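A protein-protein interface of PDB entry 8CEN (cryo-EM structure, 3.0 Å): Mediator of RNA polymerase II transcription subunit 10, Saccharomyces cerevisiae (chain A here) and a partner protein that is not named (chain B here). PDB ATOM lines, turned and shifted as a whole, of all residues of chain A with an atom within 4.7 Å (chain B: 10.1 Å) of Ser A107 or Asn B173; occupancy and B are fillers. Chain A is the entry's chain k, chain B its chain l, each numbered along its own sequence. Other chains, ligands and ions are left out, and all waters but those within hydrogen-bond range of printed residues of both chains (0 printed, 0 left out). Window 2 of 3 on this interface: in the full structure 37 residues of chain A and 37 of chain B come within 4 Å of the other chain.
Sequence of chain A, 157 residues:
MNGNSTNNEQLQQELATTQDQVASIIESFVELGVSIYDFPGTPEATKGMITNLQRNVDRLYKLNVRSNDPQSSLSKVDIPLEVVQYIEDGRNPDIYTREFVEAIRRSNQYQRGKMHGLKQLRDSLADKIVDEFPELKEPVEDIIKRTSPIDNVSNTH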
ATOM      1  N   ALA A 103      34.489 -33.875 -20.151  1.00  0.00           N
ATOM      2  CA  ALA A 103      33.039 -33.743 -20.044  1.00  0.00           C
ATOM      3  C   ALA A 103      32.563 -32.369 -20.500  1.00  0.00           C
ATOM      4  O   ALA A 103      31.464 -32.255 -21.060  1.00  0.00           O
ATOM      5  CB  ALA A 103      32.591 -34.013 -18.608  1.00  0.00           C
ATOM      6  N   ILE A 104      33.368 -31.328 -20.258  1.00  0.00           N
ATOM      7  CA  ILE A 104      33.085 -30.005 -20.822  1.00  0.00           C
ATOM      8  C   ILE A 104      33.002 -30.085 -22.340  1.00  0.00           C
ATOM      9  O   ILE A 104      32.041 -29.608 -22.959  1.00  0.00           O
ATOM     10  CB  ILE A 104      34.159 -28.985 -20.406  1.00  0.00           C
ATOM     11  CG1 ILE A 104      34.248 -28.852 -18.896  1.00  0.00           C
ATOM     12  CG2 ILE A 104      33.861 -27.626 -21.027  1.00  0.00           C
ATOM     13  CD1 ILE A 104      33.005 -28.377 -18.288  1.00  0.00           C
ATOM     14  N   ARG A 105      34.015 -30.700 -22.959  1.00  0.00           N
ATOM     15  CA  ARG A 105      34.018 -30.790 -24.418  1.00  0.00           C
ATOM     16  C   ARG A 105      32.921 -31.715 -24.936  1.00  0.00           C
ATOM     17  O   ARG A 105      32.361 -31.458 -26.008  1.00  0.00           O
ATOM     18  CB  ARG A 105      35.392 -31.226 -24.930  1.00  0.00           C
ATOM     19  CG  ARG A 105      36.543 -30.442 -24.315  1.00  0.00           C
ATOM     20  CD  ARG A 105      37.857 -30.643 -25.056  1.00  0.00           C
ATOM     21  NE  ARG A 105      37.958 -29.773 -26.223  1.00  0.00           N
ATOM     22  CZ  ARG A 105      39.095 -29.456 -26.828  1.00  0.00           C
ATOM     23  NH1 ARG A 105      40.257 -29.925 -26.406  1.00  0.00           N
ATOM     24  NH2 ARG A 105      39.065 -28.644 -27.881  1.00  0.00           N
ATOM     25  N   ARG A 106      32.577 -32.771 -24.186  1.00  0.00           N
ATOM     26  CA  ARG A 106      31.452 -33.628 -24.562  1.00  0.00           C
ATOM     27  C   ARG A 106      30.141 -32.859 -24.573  1.00  0.00           C
ATOM     28  O   ARG A 106      29.350 -32.988 -25.510  1.00  0.00           O
ATOM     29  CB  ARG A 106      31.315 -34.834 -23.631  1.00  0.00           C
ATOM     30  CG  ARG A 106      32.438 -35.827 -23.635  1.00  0.00           C
ATOM     31  CD  ARG A 106      32.463 -36.505 -24.967  1.00  0.00           C
ATOM     32  NE  ARG A 106      31.213 -37.197 -25.226  1.00  0.00           N
ATOM     33  CZ  ARG A 106      30.930 -38.430 -24.836  1.00  0.00           C
ATOM     34  NH1 ARG A 106      31.794 -39.154 -24.145  1.00  0.00           N
ATOM     35  NH2 ARG A 106      29.747 -38.952 -25.149  1.00  0.00           N
ATOM     36  N   SER A 107      29.878 -32.077 -23.523  1.00  0.00           N
ATOM     37  CA  SER A 107      28.622 -31.339 -23.477  1.00  0.00           C
ATOM     38  C   SER A 107      28.586 -30.246 -24.536  1.00  0.00           C
ATOM     39  O   SER A 107      27.530 -30.010 -25.136  1.00  0.00           O
ATOM     40  CB  SER A 107      28.397 -30.754 -22.086  1.00  0.00           C
ATOM     41  OG  SER A 107      27.030 -30.430 -21.910  1.00  0.00           O
ATOM     42  N   ASN A 108      29.731 -29.608 -24.806  1.00  0.00           N
ATOM     43  CA  ASN A 108      29.790 -28.600 -25.861  1.00  0.00           C
ATOM     44  C   ASN A 108      29.502 -29.213 -27.227  1.00  0.00           C
ATOM     45  O   ASN A 108      28.689 -28.689 -27.997  1.00  0.00           O
ATOM     46  CB  ASN A 108      31.156 -27.914 -25.850  1.00  0.00           C
ATOM     47  CG  ASN A 108      31.245 -26.781 -26.850  1.00  0.00           C
ATOM     48  OD1 ASN A 108      32.261 -26.608 -27.523  1.00  0.00           O
ATOM     49  ND2 ASN A 108      30.176 -26.001 -26.956  1.00  0.00           N
ATOM     50  N   GLN A 109      30.132 -30.354 -27.528  1.00  0.00           N
ATOM     51  CA  GLN A 109      29.910 -31.012 -28.812  1.00  0.00           C
ATOM     52  C   GLN A 109      28.507 -31.595 -28.924  1.00  0.00           C
ATOM     53  O   GLN A 109      27.924 -31.582 -30.010  1.00  0.00           O
ATOM     54  CB  GLN A 109      30.954 -32.103 -29.024  1.00  0.00           C
ATOM     55  CG  GLN A 109      32.358 -31.576 -29.245  1.00  0.00           C
ATOM     56  CD  GLN A 109      33.376 -32.689 -29.339  1.00  0.00           C
ATOM     57  OE1 GLN A 109      33.021 -33.859 -29.476  1.00  0.00           O
ATOM     58  NE2 GLN A 109      34.652 -32.331 -29.268  1.00  0.00           N
ATOM     59  N   TYR A 110      27.945 -32.093 -27.821  1.00  0.00           N
ATOM     60  CA  TYR A 110      26.605 -32.670 -27.851  1.00  0.00           C
ATOM     61  C   TYR A 110      25.556 -31.586 -28.077  1.00  0.00           C
ATOM     62  O   TYR A 110      24.624 -31.758 -28.874  1.00  0.00           O
ATOM     63  CB  TYR A 110      26.355 -33.428 -26.546  1.00  0.00           C
ATOM     64  CG  TYR A 110      25.122 -34.301 -26.512  1.00  0.00           C
ATOM     65  CD1 TYR A 110      25.065 -35.482 -27.244  1.00  0.00           C
ATOM     66  CD2 TYR A 110      24.032 -33.970 -25.717  1.00  0.00           C
ATOM     67  CE1 TYR A 110      23.949 -36.296 -27.202  1.00  0.00           C
ATOM     68  CE2 TYR A 110      22.912 -34.779 -25.670  1.00  0.00           C
ATOM     69  CZ  TYR A 110      22.875 -35.937 -26.415  1.00  0.00           C
ATOM     70  OH  TYR A 110      21.758 -36.741 -26.370  1.00  0.00           O
ATOM     71  N   GLN A 111      25.715 -30.440 -27.404  1.00  0.00           N
ATOM     72  CA  GLN A 111      24.804 -29.324 -27.626  1.00  0.00           C
ATOM     73  C   GLN A 111      24.985 -28.724 -29.017  1.00  0.00           C
ATOM     74  O   GLN A 111      24.004 -28.299 -29.636  1.00  0.00           O
ATOM     75  CB  GLN A 111      25.013 -28.261 -26.545  1.00  0.00           C
ATOM     76  CG  GLN A 111      23.992 -27.129 -26.541  1.00  0.00           C
ATOM     77  CD  GLN A 111      22.650 -27.518 -25.933  1.00  0.00           C
ATOM     78  OE1 GLN A 111      22.436 -28.663 -25.534  1.00  0.00           O
ATOM     79  NE2 GLN A 111      21.741 -26.554 -25.858  1.00  0.00           N
ATOM     80  N   LYS A 114      23.116 -30.935 -31.276  1.00  0.00           N
ATOM     81  CA  LYS A 114      21.709 -30.546 -31.174  1.00  0.00           C
ATOM     82  C   LYS A 114      21.410 -29.341 -32.055  1.00  0.00           C
ATOM     83  O   LYS A 114      20.426 -29.333 -32.805  1.00  0.00           O
ATOM     84  CB  LYS A 114      21.343 -30.212 -29.727  1.00  0.00           C
ATOM     85  CG  LYS A 114      21.335 -31.356 -28.746  1.00  0.00           C
ATOM     86  CD  LYS A 114      20.847 -30.862 -27.393  1.00  0.00           C
ATOM     87  CE  LYS A 114      20.908 -31.942 -26.335  1.00  0.00           C
ATOM     88  NZ  LYS A 114      19.945 -33.043 -26.593  1.00  0.00           N
ATOM     89  N   LEU B 162      34.981 -23.305 -14.316  1.00  0.00           N
ATOM     90  CA  LEU B 162      34.765 -24.649 -14.856  1.00  0.00           C
ATOM     91  C   LEU B 162      33.454 -25.262 -14.361  1.00  0.00           C
ATOM     92  O   LEU B 162      32.653 -25.786 -15.152  1.00  0.00           O
ATOM     93  CB  LEU B 162      35.958 -25.523 -14.466  1.00  0.00           C
ATOM     94  CG  LEU B 162      36.123 -26.981 -14.886  1.00  0.00           C
ATOM     95  CD1 LEU B 162      36.229 -27.164 -16.371  1.00  0.00           C
ATOM     96  CD2 LEU B 162      37.348 -27.562 -14.200  1.00  0.00           C
ATOM     97  N   ASP B 164      30.772 -23.781 -12.962  1.00  0.00           N
ATOM     98  CA  ASP B 164      29.621 -23.025 -13.445  1.00  0.00           C
ATOM     99  C   ASP B 164      29.367 -23.273 -14.924  1.00  0.00           C
ATOM    100  O   ASP B 164      28.206 -23.341 -15.347  1.00  0.00           O
ATOM    101  CB  ASP B 164      29.825 -21.532 -13.194  1.00  0.00           C
ATOM    102  CG  ASP B 164      30.006 -21.209 -11.728  1.00  0.00           C
ATOM    103  OD1 ASP B 164      29.590 -22.028 -10.881  1.00  0.00           O
ATOM    104  OD2 ASP B 164      30.574 -20.140 -11.422  1.00  0.00           O
ATOM    105  N   LEU B 165      30.434 -23.425 -15.715  1.00  0.00           N
ATOM    106  CA  LEU B 165      30.279 -23.763 -17.124  1.00  0.00           C
ATOM    107  C   LEU B 165      29.584 -25.104 -17.298  1.00  0.00           C
ATOM    108  O   LEU B 165      28.695 -25.241 -18.144  1.00  0.00           O
ATOM    109  CB  LEU B 165      31.642 -23.776 -17.815  1.00  0.00           C
ATOM    110  CG  LEU B 165      31.606 -23.815 -19.344  1.00  0.00           C
ATOM    111  CD1 LEU B 165      30.648 -22.764 -19.875  1.00  0.00           C
ATOM    112  CD2 LEU B 165      32.998 -23.620 -19.924  1.00  0.00           C
ATOM    113  N   LEU B 166      29.951 -26.102 -16.492  1.00  0.00           N
ATOM    114  CA  LEU B 166      29.332 -27.402 -16.725  1.00  0.00           C
ATOM    115  C   LEU B 166      27.908 -27.475 -16.174  1.00  0.00           C
ATOM    116  O   LEU B 166      27.059 -28.173 -16.747  1.00  0.00           O
ATOM    117  CB  LEU B 166      30.206 -28.515 -16.156  1.00  0.00           C
ATOM    118  CG  LEU B 166      29.707 -29.927 -16.413  1.00  0.00           C
ATOM    119  CD1 LEU B 166      29.681 -30.144 -17.908  1.00  0.00           C
ATOM    120  CD2 LEU B 166      30.708 -30.854 -15.842  1.00  0.00           C
ATOM    121  N   ASN B 167      27.604 -26.745 -15.094  1.00  0.00           N
ATOM    122  CA  ASN B 167      26.207 -26.647 -14.670  1.00  0.00           C
ATOM    123  C   ASN B 167      25.359 -25.913 -15.708  1.00  0.00           C
ATOM    124  O   ASN B 167      24.210 -26.302 -15.969  1.00  0.00           O
ATOM    125  CB  ASN B 167      26.097 -25.973 -13.301  1.00  0.00           C
ATOM    126  CG  ASN B 167      26.717 -26.803 -12.191  1.00  0.00           C
ATOM    127  OD1 ASN B 167      27.697 -26.402 -11.570  1.00  0.00           O
ATOM    128  ND2 ASN B 167      26.143 -27.974 -11.942  1.00  0.00           N
ATOM    129  N   TRP B 168      25.916 -24.864 -16.324  1.00  0.00           N
ATOM    130  CA  TRP B 168      25.243 -24.205 -17.439  1.00  0.00           C
ATOM    131  C   TRP B 168      25.045 -25.167 -18.604  1.00  0.00           C
ATOM    132  O   TRP B 168      24.017 -25.117 -19.293  1.00  0.00           O
ATOM    133  CB  TRP B 168      26.048 -22.979 -17.874  1.00  0.00           C
ATOM    134  CG  TRP B 168      25.463 -22.231 -19.034  1.00  0.00           C
ATOM    135  CD1 TRP B 168      24.600 -21.175 -18.978  1.00  0.00           C
ATOM    136  CD2 TRP B 168      25.714 -22.471 -20.423  1.00  0.00           C
ATOM    137  NE1 TRP B 168      24.292 -20.749 -20.247  1.00  0.00           N
ATOM    138  CE2 TRP B 168      24.962 -21.529 -21.152  1.00  0.00           C
ATOM    139  CE3 TRP B 168      26.497 -23.396 -21.122  1.00  0.00           C
ATOM    140  CZ2 TRP B 168      24.972 -21.484 -22.544  1.00  0.00           C
ATOM    141  CZ3 TRP B 168      26.502 -23.350 -22.502  1.00  0.00           C
ATOM    142  CH2 TRP B 168      25.746 -22.401 -23.199  1.00  0.00           C
ATOM    143  N   PHE B 169      26.020 -26.049 -18.837  1.00  0.00           N
ATOM    144  CA  PHE B 169      25.891 -27.055 -19.886  1.00  0.00           C
ATOM    145  C   PHE B 169      24.764 -28.037 -19.594  1.00  0.00           C
ATOM    146  O   PHE B 169      24.043 -28.445 -20.509  1.00  0.00           O
ATOM    147  CB  PHE B 169      27.207 -27.803 -20.068  1.00  0.00           C
ATOM    148  CG  PHE B 169      28.097 -27.200 -21.105  1.00  0.00           C
ATOM    149  CD1 PHE B 169      27.640 -27.031 -22.399  1.00  0.00           C
ATOM    150  CD2 PHE B 169      29.394 -26.828 -20.798  1.00  0.00           C
ATOM    151  CE1 PHE B 169      28.446 -26.475 -23.362  1.00  0.00           C
ATOM    152  CE2 PHE B 169      30.210 -26.277 -21.762  1.00  0.00           C
ATOM    153  CZ  PHE B 169      29.737 -26.106 -23.046  1.00  0.00           C
ATOM    154  N   ARG B 170      24.618 -28.448 -18.333  1.00  0.00           N
ATOM    155  CA  ARG B 170      23.486 -29.295 -17.958  1.00  0.00           C
ATOM    156  C   ARG B 170      22.153 -28.591 -18.172  1.00  0.00           C
ATOM    157  O   ARG B 170      21.201 -29.200 -18.681  1.00  0.00           O
ATOM    158  CB  ARG B 170      23.629 -29.765 -16.511  1.00  0.00           C
ATOM    159  CG  ARG B 170      24.842 -30.647 -16.231  1.00  0.00           C
ATOM    160  CD  ARG B 170      24.646 -32.088 -16.757  1.00  0.00           C
ATOM    161  NE  ARG B 170      24.748 -32.264 -18.202  1.00  0.00           N
ATOM    162  CZ  ARG B 170      25.887 -32.307 -18.879  1.00  0.00           C
ATOM    163  NH1 ARG B 170      27.056 -32.194 -18.272  1.00  0.00           N
ATOM    164  NH2 ARG B 170      25.852 -32.471 -20.198  1.00  0.00           N
ATOM    165  N   THR B 171      22.070 -27.307 -17.810  1.00  0.00           N
ATOM    166  CA  THR B 171      20.839 -26.554 -18.055  1.00  0.00           C
ATOM    167  C   THR B 171      20.521 -26.482 -19.548  1.00  0.00           C
ATOM    168  O   THR B 171      19.375 -26.696 -19.962  1.00  0.00           O
ATOM    169  CB  THR B 171      20.936 -25.147 -17.465  1.00  0.00           C
ATOM    170  OG1 THR B 171      22.003 -24.429 -18.099  1.00  0.00           O
ATOM    171  CG2 THR B 171      21.160 -25.201 -15.962  1.00  0.00           C
ATOM    172  N   THR B 172      21.535 -26.214 -20.375  1.00  0.00           N
ATOM    173  CA  THR B 172      21.291 -26.078 -21.808  1.00  0.00           C
ATOM    174  C   THR B 172      20.986 -27.414 -22.472  1.00  0.00           C
ATOM    175  O   THR B 172      20.203 -27.461 -23.427  1.00  0.00           O
ATOM    176  CB  THR B 172      22.484 -25.418 -22.486  1.00  0.00           C
ATOM    177  OG1 THR B 172      23.681 -26.117 -22.134  1.00  0.00           O
ATOM    178  CG2 THR B 172      22.590 -23.995 -22.023  1.00  0.00           C
ATOM    179  N   ASN B 173      21.589 -28.504 -21.992  1.00  0.00           N
ATOM    180  CA  ASN B 173      21.236 -29.818 -22.513  1.00  0.00           C
ATOM    181  C   ASN B 173      19.850 -30.243 -22.055  1.00  0.00           C
ATOM    182  O   ASN B 173      19.216 -31.083 -22.702  1.00  0.00           O
ATOM    183  CB  ASN B 173      22.275 -30.855 -22.088  1.00  0.00           C
ATOM    184  CG  ASN B 173      23.626 -30.622 -22.729  1.00  0.00           C
ATOM    185  OD1 ASN B 173      24.663 -30.907 -22.130  1.00  0.00           O
ATOM    186  ND2 ASN B 173      23.624 -30.105 -23.952  1.00  0.00           N
ATOM    187  N   MET B 174      19.367 -29.685 -20.946  1.00  0.00           N
ATOM    188  CA  MET B 174      18.017 -29.997 -20.499  1.00  0.00           C
ATOM    189  C   MET B 174      16.942 -29.107 -21.115  1.00  0.00           C
ATOM    190  O   MET B 174      15.766 -29.483 -21.073  1.00  0.00           O
ATOM    191  CB  MET B 174      17.942 -29.905 -18.968  1.00  0.00           C
ATOM    192  CG  MET B 174      18.437 -31.142 -18.187  1.00  0.00           C
ATOM    193  SD  MET B 174      18.060 -32.868 -18.648  1.00  0.00           S
ATOM    194  CE  MET B 174      16.368 -32.861 -19.262  1.00  0.00           C
ATOM    195  N   ASN B 175      17.309 -27.944 -21.671  1.00  0.00           N
ATOM    196  CA  ASN B 175      16.297 -27.033 -22.218  1.00  0.00           C
ATOM    197  C   ASN B 175      15.549 -27.628 -23.411  1.00  0.00           C
ATOM    198  O   ASN B 175      14.349 -27.384 -23.572  1.00  0.00           O
ATOM    199  CB  ASN B 175      16.917 -25.692 -22.612  1.00  0.00           C
ATOM    200  CG  ASN B 175      17.461 -24.927 -21.428  1.00  0.00           C
ATOM    201  OD1 ASN B 175      18.519 -24.306 -21.508  1.00  0.00           O
ATOM    202  ND2 ASN B 175      16.735 -24.964 -20.317  1.00  0.00           N
ATOM    203  N   VAL B 176      16.233 -28.393 -24.266  1.00  0.00           N
ATOM    204  CA  VAL B 176      15.567 -28.937 -25.448  1.00  0.00           C
ATOM    205  C   VAL B 176      14.546 -29.998 -25.047  1.00  0.00           C
ATOM    206  O   VAL B 176      13.414 -30.023 -25.558  1.00  0.00           O
ATOM    207  CB  VAL B 176      16.603 -29.492 -26.441  1.00  0.00           C
ATOM    208  CG1 VAL B 176      15.918 -29.986 -27.706  1.00  0.00           C
ATOM    209  CG2 VAL B 176      17.648 -28.437 -26.767  1.00  0.00           C
ATOM    210  N   ASN B 177      14.918 -30.877 -24.112  1.00  0.00           N
ATOM    211  CA  ASN B 177      13.964 -31.848 -23.588  1.00  0.00           C
ATOM    212  C   ASN B 177      12.841 -31.167 -22.818  1.00  0.00           C
ATOM    213  O   ASN B 177      11.706 -31.650 -22.828  1.00  0.00           O
ATOM    214  CB  ASN B 177      14.678 -32.867 -22.701  1.00  0.00           C
ATOM    215  CG  ASN B 177      14.026 -34.238 -22.748  1.00  0.00           C
ATOM    216  OD1 ASN B 177      12.845 -34.366 -23.070  1.00  0.00           O
ATOM    217  ND2 ASN B 177      14.798 -35.269 -22.429  1.00  0.00           N
ATOM    218  N   ASN B 178      13.133 -30.041 -22.158  1.00  0.00           N
ATOM    219  CA  ASN B 178      12.079 -29.275 -21.501  1.00  0.00           C
ATOM    220  C   ASN B 178      11.096 -28.700 -22.511  1.00  0.00           C
ATOM    221  O   ASN B 178       9.888 -28.672 -22.260  1.00  0.00           O
ATOM    222  CB  ASN B 178      12.691 -28.163 -20.650  1.00  0.00           C
ATOM    223  CG  ASN B 178      13.323 -28.688 -19.379  1.00  0.00           C
ATOM    224  OD1 ASN B 178      12.885 -29.695 -18.823  1.00  0.00           O
ATOM    225  ND2 ASN B 178      14.370 -28.013 -18.919  1.00  0.00           N
ATOM    226  N   CYS B 179      11.594 -28.228 -23.656  1.00  0.00           N
ATOM    227  CA  CYS B 179      10.708 -27.752 -24.718  1.00  0.00           C
ATOM    228  C   CYS B 179       9.858 -28.887 -25.275  1.00  0.00           C
ATOM    229  O   CYS B 179       8.669 -28.700 -25.573  1.00  0.00           O
ATOM    230  CB  CYS B 179      11.524 -27.097 -25.832  1.00  0.00           C
ATOM    231  SG  CYS B 179      10.540 -26.500 -27.226  1.00  0.00           S
ATOM    232  N   ILE B 180      10.455 -30.072 -25.419  1.00  0.00           N
ATOM    233  CA  ILE B 180       9.712 -31.245 -25.879  1.00  0.00           C
ATOM    234  C   ILE B 180       8.608 -31.606 -24.888  1.00  0.00           C
ATOM    235  O   ILE B 180       7.464 -31.873 -25.275  1.00  0.00           O
ATOM    236  CB  ILE B 180      10.675 -32.422 -26.110  1.00  0.00           C
ATOM    237  CG1 ILE B 180      11.488 -32.192 -27.383  1.00  0.00           C
ATOM    238  CG2 ILE B 180       9.923 -33.737 -26.176  1.00  0.00           C
ATOM    239  CD1 ILE B 180      12.663 -33.112 -27.514  1.00  0.00           C
ATOM    240  N   TRP B 181       8.930 -31.603 -23.592  1.00  0.00           N
ATOM    241  CA  TRP B 181       7.927 -31.908 -22.575  1.00  0.00           C
ATOM    242  C   TRP B 181       6.876 -30.809 -22.464  1.00  0.00           C
ATOM    243  O   TRP B 181       5.729 -31.089 -22.107  1.00  0.00           O
ATOM    244  CB  TRP B 181       8.604 -32.145 -21.223  1.00  0.00           C
ATOM    245  CG  TRP B 181       9.238 -33.505 -21.099  1.00  0.00           C
ATOM    246  CD1 TRP B 181      10.566 -33.778 -20.953  1.00  0.00           C
ATOM    247  CD2 TRP B 181       8.565 -34.773 -21.083  1.00  0.00           C
ATOM    248  NE1 TRP B 181      10.766 -35.133 -20.867  1.00  0.00           N
ATOM    249  CE2 TRP B 181       9.554 -35.767 -20.940  1.00  0.00           C
ATOM    250  CE3 TRP B 181       7.226 -35.164 -21.179  1.00  0.00           C
ATOM    251  CZ2 TRP B 181       9.247 -37.125 -20.892  1.00  0.00           C
ATOM    252  CZ3 TRP B 181       6.924 -36.514 -21.130  1.00  0.00           C
ATOM    253  CH2 TRP B 181       7.930 -37.477 -20.989  1.00  0.00           C
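Hydrophobic or aromatic side chains of chain A within 4 Å of the printed part of chain B: Ile A104.
Along chain A the printed residues that touch a printed residue of chain B span positions 104 to 111.
Of the 19 printed residues of chain B, 6 touch a printed residue of chain A.
Hydrophobic or aromatic side chains of chain B within 4 Å of the printed part of chain A: Leu B162, Leu B166 and Phe B169.
Among the printed residues, no Asp or Glu carboxylate lies within 4 Å of a Lys or Arg side-chain nitrogen of the other chain.
The guanidinium group of Arg B170 sits at hydrogen-bond distance from the side-chain hydroxyl of Ser A107.
The side-chain amide oxygen of Asn B173 lies within hydrogen-bond range of the side-chain hydroxyl of Ser A107.
The side-chain amide nitrogen (NE2) of Gln A111 sits at hydrogen-bond distance from the backbone carbonyl oxygen (O) of Thr B172 (3.0 Å).
The side-chain amide oxygen of Gln A111 is in hydrogen-bond range of the side-chain amide nitrogen of Asn B173, at 2.4 Å.
Among the printed residues, merely in contact across the chains: Ile A104 with Leu B162 (3.6 Å), Ile A104 with Leu B166 (3.5 Å), Ile A104 with Phe B169 (3.96 Å), Ser A107 with Phe B169 (3.2 Å) and Asn A108 with Phe B169 (3.5 Å).
The side-chain hydroxyl (OG1) of Thr B172 is in hydrogen-bond range of the backbone carbonyl oxygen (O) of Trp B168 (3.0 Å).
The backbone carbonyl oxygen (O) of Phe B169 sits at hydrogen-bond distance from the side-chain hydroxyl (OG1) of Thr B172 (2.9 Å).
The backbone carbonyl oxygen (O) of Phe B169 lies close to the side-chain amide oxygen (OD1) of Asn B173 (3.0 Å).
NH2 of Arg B170 lies within hydrogen-bond range of OD1 of Asn B173 (2.8 Å).
Printed residues of chain B within 4 Å of Ser A107: Phe B169, Arg B170 and Asn B173.
Asn B173 touches just these residues of chain A: Ser A107 (2.4 Å) and Gln A111 (2.4 Å).
No residue of chain B comes within 4 Å of Ala A103.
Asn A108 touches just one residue of chain B: Phe B169.
Printed residues of chain A within 4 Å of Arg B170: Ser A107 (2.9 Å).
Printed residues of chain A within 4 Å of Phe B169: Ile A104, Ser A107 and Asn A108.
Of the printed residues of chain B, Ile A104 touches Leu B162, Leu B166 and Phe B169.
Printed residues of chain A within 4 Å of Thr B172: Gln A111.
Of the printed residues of chain A, Leu B166 touches Ile A104 (3.5 Å).
Asn B175 touches none of the printed residues of chain A.
The nearest printed residue of chain A that does not touch Leu B162 is Ala A103 (7.6 Å).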
